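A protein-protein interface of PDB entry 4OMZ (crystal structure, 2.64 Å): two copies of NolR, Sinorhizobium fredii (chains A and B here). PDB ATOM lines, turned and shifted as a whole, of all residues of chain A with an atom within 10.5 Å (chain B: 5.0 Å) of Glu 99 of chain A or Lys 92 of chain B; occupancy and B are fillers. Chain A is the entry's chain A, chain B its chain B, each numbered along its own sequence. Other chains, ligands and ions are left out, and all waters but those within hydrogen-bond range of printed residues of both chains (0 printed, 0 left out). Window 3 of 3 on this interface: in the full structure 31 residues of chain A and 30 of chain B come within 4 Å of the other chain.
Hydrophobic or aromatic side chains of chain A within 4 Å of the printed part of chain B: Ile 93, Ala 96 and Ile 100. Hydrophobic or aromatic side chains of chain B within 4 Å of the printed part of chain A: Ile 93 and Ala 96. Along chain B the printed residues that touch a printed residue of chain A span positions 89 to 96. Among the printed residues, no Asp or Glu carboxylate lies within 4 Å of a Lys or Arg side-chain nitrogen of the other chain.
The side-chain carboxylate (OD1) of Asp 88 of chain B lies within salt-bridge range of the side-chain amino group (NZ) of Lys 92 of chain B, 2.7 Å away.
Ile 93 of chain A touches Ala 96 of chain B, and with the chains exchanged Ala 96 of chain A touches Ile 93 of chain B. Positions printed for both chains: 89, 91, 92, 93, 94, 95 and 96. Of the 5 pairs that touch across the chains among the printed residues, 2 have their exchanged pair printed and touching as well.
Ile 93 of chain A touches Ala 96 of chain B (CD1 to CB, 3.8 Å). Ala 96 of chain A touches Ile 93 of chain B (CB to CD1, 3.7 Å). Lys 92 of chain B touches Glu 99 of chain A (CE to OE1, 3.7 Å). Ile 100 of chain A touches Ser 89 of chain B (CG2 to OG, 3.4 Å). Lys 92 of chain B touches Ile 100 of chain A.
Printed residues of chain B within 4 Å of Glu 99 of chain A: Lys 92. Of the printed residues of chain A, Lys 92 of chain B touches Glu 99 (3.7 Å) and Ile 100 (3.7 Å). Asp 88 of chain B touches none of the printed residues of chain A. Of the printed residues of chain A, Ile 93 of chain B touches Ala 96. No residue of chain A comes within 4 Å of Gly 95 of chain B. Of chain A, only Ile 93 comes within 4 Å of Ala 96 of chain B. Of the printed residues of chain B, Ala 96 of chain A touches Ile 93. Of the printed residues of chain B, Ile 100 of chain A touches Ser 89 and Lys 92. Gly 95 of chain A touches none of the printed residues of chain B.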
ATOM      1  N   PHE A  22      -3.044  35.715 -28.592  1.00  0.00           N
ATOM      2  CA  PHE A  22      -4.106  35.917 -27.608  1.00  0.00           C
ATOM      3  C   PHE A  22      -3.864  35.125 -26.306  1.00  0.00           C
ATOM      4  O   PHE A  22      -3.866  35.688 -25.187  1.00  0.00           O
ATOM      5  CB  PHE A  22      -5.435  35.524 -28.243  1.00  0.00           C
ATOM      6  CG  PHE A  22      -6.529  35.239 -27.264  1.00  0.00           C
ATOM      7  CD1 PHE A  22      -7.030  36.232 -26.442  1.00  0.00           C
ATOM      8  CD2 PHE A  22      -7.066  33.963 -27.175  1.00  0.00           C
ATOM      9  CE1 PHE A  22      -8.050  35.957 -25.548  1.00  0.00           C
ATOM     10  CE2 PHE A  22      -8.086  33.682 -26.283  1.00  0.00           C
ATOM     11  CZ  PHE A  22      -8.578  34.680 -25.468  1.00  0.00           C
ATOM     12  N   LEU A  23      -3.630  33.822 -26.452  1.00  0.00           N
ATOM     13  CA  LEU A  23      -3.401  32.962 -25.291  1.00  0.00           C
ATOM     14  C   LEU A  23      -2.184  33.431 -24.509  1.00  0.00           C
ATOM     15  O   LEU A  23      -2.147  33.349 -23.283  1.00  0.00           O
ATOM     16  CB  LEU A  23      -3.193  31.512 -25.709  1.00  0.00           C
ATOM     17  CG  LEU A  23      -4.403  30.747 -26.217  1.00  0.00           C
ATOM     18  CD1 LEU A  23      -3.988  29.335 -26.582  1.00  0.00           C
ATOM     19  CD2 LEU A  23      -5.473  30.756 -25.150  1.00  0.00           C
ATOM     20  N   SER A  89     -13.708  36.843 -25.934  1.00  0.00           N
ATOM     21  CA  SER A  89     -12.607  35.880 -25.929  1.00  0.00           C
ATOM     22  C   SER A  89     -12.146  35.532 -24.513  1.00  0.00           C
ATOM     23  O   SER A  89     -12.076  34.351 -24.132  1.00  0.00           O
ATOM     24  CB  SER A  89     -11.423  36.432 -26.719  1.00  0.00           C
ATOM     25  OG  SER A  89     -11.754  36.611 -28.081  1.00  0.00           O
ATOM     26  N   MET A  91     -13.696  36.000 -21.776  1.00  0.00           N
ATOM     27  CA  MET A  91     -14.761  35.336 -21.045  1.00  0.00           C
ATOM     28  C   MET A  91     -14.886  33.863 -21.420  1.00  0.00           C
ATOM     29  O   MET A  91     -15.154  33.026 -20.557  1.00  0.00           O
ATOM     30  CB  MET A  91     -16.090  36.061 -21.262  1.00  0.00           C
ATOM     31  CG  MET A  91     -16.286  37.205 -20.284  1.00  0.00           C
ATOM     32  SD  MET A  91     -17.527  38.402 -20.792  1.00  0.00           S
ATOM     33  CE  MET A  91     -16.697  39.910 -20.306  1.00  0.00           C
ATOM     34  N   LYS A  92     -14.675  33.535 -22.689  1.00  0.00           N
ATOM     35  CA  LYS A  92     -14.740  32.138 -23.099  1.00  0.00           C
ATOM     36  C   LYS A  92     -13.592  31.335 -22.495  1.00  0.00           C
ATOM     37  O   LYS A  92     -13.791  30.205 -22.034  1.00  0.00           O
ATOM     38  CB  LYS A  92     -14.737  32.015 -24.621  1.00  0.00           C
ATOM     39  CG  LYS A  92     -16.107  32.262 -25.235  1.00  0.00           C
ATOM     40  CD  LYS A  92     -16.032  32.531 -26.727  1.00  0.00           C
ATOM     41  CE  LYS A  92     -17.420  32.588 -27.325  1.00  0.00           C
ATOM     42  NZ  LYS A  92     -17.793  31.294 -27.950  1.00  0.00           N
ATOM     43  N   ILE A  93     -12.394  31.913 -22.478  1.00  0.00           N
ATOM     44  CA  ILE A  93     -11.262  31.198 -21.894  1.00  0.00           C
ATOM     45  C   ILE A  93     -11.446  31.038 -20.384  1.00  0.00           C
ATOM     46  O   ILE A  93     -11.198  29.963 -19.843  1.00  0.00           O
ATOM     47  CB  ILE A  93      -9.925  31.894 -22.192  1.00  0.00           C
ATOM     48  CG1 ILE A  93      -9.656  31.872 -23.699  1.00  0.00           C
ATOM     49  CG2 ILE A  93      -8.787  31.200 -21.460  1.00  0.00           C
ATOM     50  CD1 ILE A  93      -9.649  30.485 -24.294  1.00  0.00           C
ATOM     51  N   LEU A  94     -11.903  32.094 -19.714  1.00  0.00           N
ATOM     52  CA  LEU A  94     -12.176  32.018 -18.279  1.00  0.00           C
ATOM     53  C   LEU A  94     -13.252  30.977 -18.008  1.00  0.00           C
ATOM     54  O   LEU A  94     -13.228  30.323 -16.977  1.00  0.00           O
ATOM     55  CB  LEU A  94     -12.608  33.374 -17.704  1.00  0.00           C
ATOM     56  CG  LEU A  94     -11.599  34.515 -17.524  1.00  0.00           C
ATOM     57  CD1 LEU A  94     -12.260  35.677 -16.796  1.00  0.00           C
ATOM     58  CD2 LEU A  94     -10.381  34.057 -16.757  1.00  0.00           C
ATOM     59  N   GLY A  95     -14.202  30.839 -18.928  1.00  0.00           N
ATOM     60  CA  GLY A  95     -15.240  29.832 -18.800  1.00  0.00           C
ATOM     61  C   GLY A  95     -14.635  28.442 -18.870  1.00  0.00           C
ATOM     62  O   GLY A  95     -14.952  27.561 -18.064  1.00  0.00           O
ATOM     63  N   ALA A  96     -13.758  28.249 -19.852  1.00  0.00           N
ATOM     64  CA  ALA A  96     -13.055  26.984 -20.004  1.00  0.00           C
ATOM     65  C   ALA A  96     -12.274  26.631 -18.741  1.00  0.00           C
ATOM     66  O   ALA A  96     -12.436  25.547 -18.194  1.00  0.00           O
ATOM     67  CB  ALA A  96     -12.129  27.045 -21.199  1.00  0.00           C
ATOM     68  N   LEU A  97     -11.460  27.565 -18.258  1.00  0.00           N
ATOM     69  CA  LEU A  97     -10.661  27.345 -17.055  1.00  0.00           C
ATOM     70  C   LEU A  97     -11.549  27.088 -15.852  1.00  0.00           C
ATOM     71  O   LEU A  97     -11.224  26.280 -14.993  1.00  0.00           O
ATOM     72  CB  LEU A  97      -9.740  28.536 -16.790  1.00  0.00           C
ATOM     73  CG  LEU A  97      -8.605  28.681 -17.806  1.00  0.00           C
ATOM     74  CD1 LEU A  97      -7.743  29.904 -17.507  1.00  0.00           C
ATOM     75  CD2 LEU A  97      -7.762  27.407 -17.840  1.00  0.00           C
ATOM     76  N   SER A  98     -12.664  27.802 -15.796  1.00  0.00           N
ATOM     77  CA  SER A  98     -13.656  27.620 -14.749  1.00  0.00           C
ATOM     78  C   SER A  98     -14.141  26.180 -14.734  1.00  0.00           C
ATOM     79  O   SER A  98     -14.282  25.579 -13.675  1.00  0.00           O
ATOM     80  CB  SER A  98     -14.833  28.574 -14.956  1.00  0.00           C
ATOM     81  OG  SER A  98     -15.761  28.473 -13.896  1.00  0.00           O
ATOM     82  N   GLU A  99     -14.392  25.628 -15.914  1.00  0.00           N
ATOM     83  CA  GLU A  99     -14.859  24.248 -16.003  1.00  0.00           C
ATOM     84  C   GLU A  99     -13.755  23.228 -15.722  1.00  0.00           C
ATOM     85  O   GLU A  99     -14.012  22.179 -15.135  1.00  0.00           O
ATOM     86  CB  GLU A  99     -15.475  23.990 -17.377  1.00  0.00           C
ATOM     87  CG  GLU A  99     -16.724  24.803 -17.628  1.00  0.00           C
ATOM     88  CD  GLU A  99     -17.477  24.357 -18.860  1.00  0.00           C
ATOM     89  OE1 GLU A  99     -16.910  23.579 -19.659  1.00  0.00           O
ATOM     90  OE2 GLU A  99     -18.641  24.781 -19.026  1.00  0.00           O
ATOM     91  N   ILE A 100     -12.531  23.538 -16.138  1.00  0.00           N
ATOM     92  CA  ILE A 100     -11.384  22.672 -15.882  1.00  0.00           C
ATOM     93  C   ILE A 100     -11.052  22.569 -14.392  1.00  0.00           C
ATOM     94  O   ILE A 100     -10.805  21.477 -13.880  1.00  0.00           O
ATOM     95  CB  ILE A 100     -10.127  23.178 -16.634  1.00  0.00           C
ATOM     96  CG1 ILE A 100     -10.310  23.053 -18.148  1.00  0.00           C
ATOM     97  CG2 ILE A 100      -8.880  22.430 -16.185  1.00  0.00           C
ATOM     98  CD1 ILE A 100      -9.407  23.973 -18.945  1.00  0.00           C
ATOM     99  N   TYR A 101     -11.074  23.706 -13.699  1.00  0.00           N
ATOM    100  CA  TYR A 101     -10.548  23.797 -12.336  1.00  0.00           C
ATOM    101  C   TYR A 101     -11.623  24.052 -11.281  1.00  0.00           C
ATOM    102  O   TYR A 101     -11.324  24.099 -10.086  1.00  0.00           O
ATOM    103  CB  TYR A 101      -9.494  24.903 -12.247  1.00  0.00           C
ATOM    104  CG  TYR A 101      -8.240  24.639 -13.049  1.00  0.00           C
ATOM    105  CD1 TYR A 101      -7.314  23.682 -12.644  1.00  0.00           C
ATOM    106  CD2 TYR A 101      -7.969  25.366 -14.196  1.00  0.00           C
ATOM    107  CE1 TYR A 101      -6.159  23.447 -13.379  1.00  0.00           C
ATOM    108  CE2 TYR A 101      -6.821  25.140 -14.934  1.00  0.00           C
ATOM    109  CZ  TYR A 101      -5.922  24.184 -14.525  1.00  0.00           C
ATOM    110  OH  TYR A 101      -4.786  23.978 -15.272  1.00  0.00           O
ATOM    111  N   GLY A 102     -12.868  24.208 -11.719  1.00  0.00           N
ATOM    112  CA  GLY A 102     -13.960  24.545 -10.821  1.00  0.00           C
ATOM    113  C   GLY A 102     -14.136  26.041 -10.616  1.00  0.00           C
ATOM    114  O   GLY A 102     -13.179  26.814 -10.702  1.00  0.00           O
ATOM    115  N   ALA A 103     -15.374  26.449 -10.349  1.00  0.00           N
ATOM    116  CA  ALA A 103     -15.711  27.861 -10.181  1.00  0.00           C
ATOM    117  C   ALA A 103     -15.866  28.226  -8.706  1.00  0.00           C
ATOM    118  O   ALA A 103     -15.631  29.370  -8.313  1.00  0.00           O
ATOM    119  CB  ALA A 103     -16.985  28.194 -10.944  1.00  0.00           C
ATOM    120  N   ASP B  88      -8.794  16.477 -21.586  1.00  0.00           N
ATOM    121  CA  ASP B  88     -10.068  17.180 -21.502  1.00  0.00           C
ATOM    122  C   ASP B  88      -9.835  18.697 -21.517  1.00  0.00           C
ATOM    123  O   ASP B  88     -10.570  19.452 -22.168  1.00  0.00           O
ATOM    124  CB  ASP B  88     -10.816  16.758 -20.233  1.00  0.00           C
ATOM    125  CG  ASP B  88     -12.127  17.503 -20.045  1.00  0.00           C
ATOM    126  OD1 ASP B  88     -12.147  18.501 -19.294  1.00  0.00           O
ATOM    127  OD2 ASP B  88     -13.135  17.103 -20.667  1.00  0.00           O
ATOM    128  N   SER B  89      -8.791  19.123 -20.809  1.00  0.00           N
ATOM    129  CA  SER B  89      -8.394  20.527 -20.755  1.00  0.00           C
ATOM    130  C   SER B  89      -8.077  21.082 -22.137  1.00  0.00           C
ATOM    131  O   SER B  89      -8.642  22.109 -22.562  1.00  0.00           O
ATOM    132  CB  SER B  89      -7.173  20.698 -19.848  1.00  0.00           C
ATOM    133  OG  SER B  89      -7.482  20.362 -18.509  1.00  0.00           O
ATOM    134  N   VAL B  90      -7.185  20.384 -22.839  1.00  0.00           N
ATOM    135  CA  VAL B  90      -6.773  20.798 -24.170  1.00  0.00           C
ATOM    136  C   VAL B  90      -7.999  20.927 -25.052  1.00  0.00           C
ATOM    137  O   VAL B  90      -8.142  21.909 -25.768  1.00  0.00           O
ATOM    138  CB  VAL B  90      -5.777  19.798 -24.812  1.00  0.00           C
ATOM    139  CG1 VAL B  90      -5.596  20.097 -26.290  1.00  0.00           C
ATOM    140  CG2 VAL B  90      -4.435  19.839 -24.100  1.00  0.00           C
ATOM    141  N   MET B  91      -8.911  19.963 -24.957  1.00  0.00           N
ATOM    142  CA  MET B  91     -10.116  19.987 -25.778  1.00  0.00           C
ATOM    143  C   MET B  91     -11.034  21.161 -25.450  1.00  0.00           C
ATOM    144  O   MET B  91     -11.646  21.737 -26.345  1.00  0.00           O
ATOM    145  CB  MET B  91     -10.882  18.675 -25.638  1.00  0.00           C
ATOM    146  CG  MET B  91     -10.377  17.597 -26.573  1.00  0.00           C
ATOM    147  SD  MET B  91     -10.882  15.941 -26.086  1.00  0.00           S
ATOM    148  CE  MET B  91      -9.362  15.050 -26.407  1.00  0.00           C
ATOM    149  N   LYS B  92     -11.129  21.524 -24.176  1.00  0.00           N
ATOM    150  CA  LYS B  92     -11.955  22.673 -23.813  1.00  0.00           C
ATOM    151  C   LYS B  92     -11.367  23.973 -24.358  1.00  0.00           C
ATOM    152  O   LYS B  92     -12.098  24.827 -24.878  1.00  0.00           O
ATOM    153  CB  LYS B  92     -12.121  22.772 -22.294  1.00  0.00           C
ATOM    154  CG  LYS B  92     -13.198  21.864 -21.720  1.00  0.00           C
ATOM    155  CD  LYS B  92     -13.048  21.738 -20.212  1.00  0.00           C
ATOM    156  CE  LYS B  92     -14.236  21.026 -19.592  1.00  0.00           C
ATOM    157  NZ  LYS B  92     -14.448  19.672 -20.174  1.00  0.00           N
ATOM    158  N   ILE B  93     -10.048  24.116 -24.256  1.00  0.00           N
ATOM    159  CA  ILE B  93      -9.402  25.323 -24.766  1.00  0.00           C
ATOM    160  C   ILE B  93      -9.508  25.386 -26.289  1.00  0.00           C
ATOM    161  O   ILE B  93      -9.804  26.441 -26.850  1.00  0.00           O
ATOM    162  CB  ILE B  93      -7.920  25.414 -24.336  1.00  0.00           C
ATOM    163  CG1 ILE B  93      -7.828  25.584 -22.825  1.00  0.00           C
ATOM    164  CG2 ILE B  93      -7.236  26.598 -24.999  1.00  0.00           C
ATOM    165  CD1 ILE B  93      -8.588  26.789 -22.318  1.00  0.00           C
ATOM    166  N   LEU B  94      -9.286  24.259 -26.956  1.00  0.00           N
ATOM    167  CA  LEU B  94      -9.423  24.209 -28.409  1.00  0.00           C
ATOM    168  C   LEU B  94     -10.855  24.519 -28.829  1.00  0.00           C
ATOM    169  O   LEU B  94     -11.078  25.163 -29.850  1.00  0.00           O
ATOM    170  CB  LEU B  94      -9.007  22.843 -28.962  1.00  0.00           C
ATOM    171  CG  LEU B  94      -7.516  22.502 -28.929  1.00  0.00           C
ATOM    172  CD1 LEU B  94      -7.234  21.210 -29.681  1.00  0.00           C
ATOM    173  CD2 LEU B  94      -6.676  23.643 -29.480  1.00  0.00           C
ATOM    174  N   GLY B  95     -11.823  24.077 -28.035  1.00  0.00           N
ATOM    175  CA  GLY B  95     -13.216  24.357 -28.326  1.00  0.00           C
ATOM    176  C   GLY B  95     -13.481  25.848 -28.253  1.00  0.00           C
ATOM    177  O   GLY B  95     -14.105  26.441 -29.154  1.00  0.00           O
ATOM    178  N   ALA B  96     -12.986  26.458 -27.179  1.00  0.00           N
ATOM    179  CA  ALA B  96     -13.108  27.900 -27.002  1.00  0.00           C
ATOM    180  C   ALA B  96     -12.489  28.644 -28.183  1.00  0.00           C
ATOM    181  O   ALA B  96     -13.130  29.504 -28.779  1.00  0.00           O
ATOM    182  CB  ALA B  96     -12.461  28.328 -25.710  1.00  0.00           C
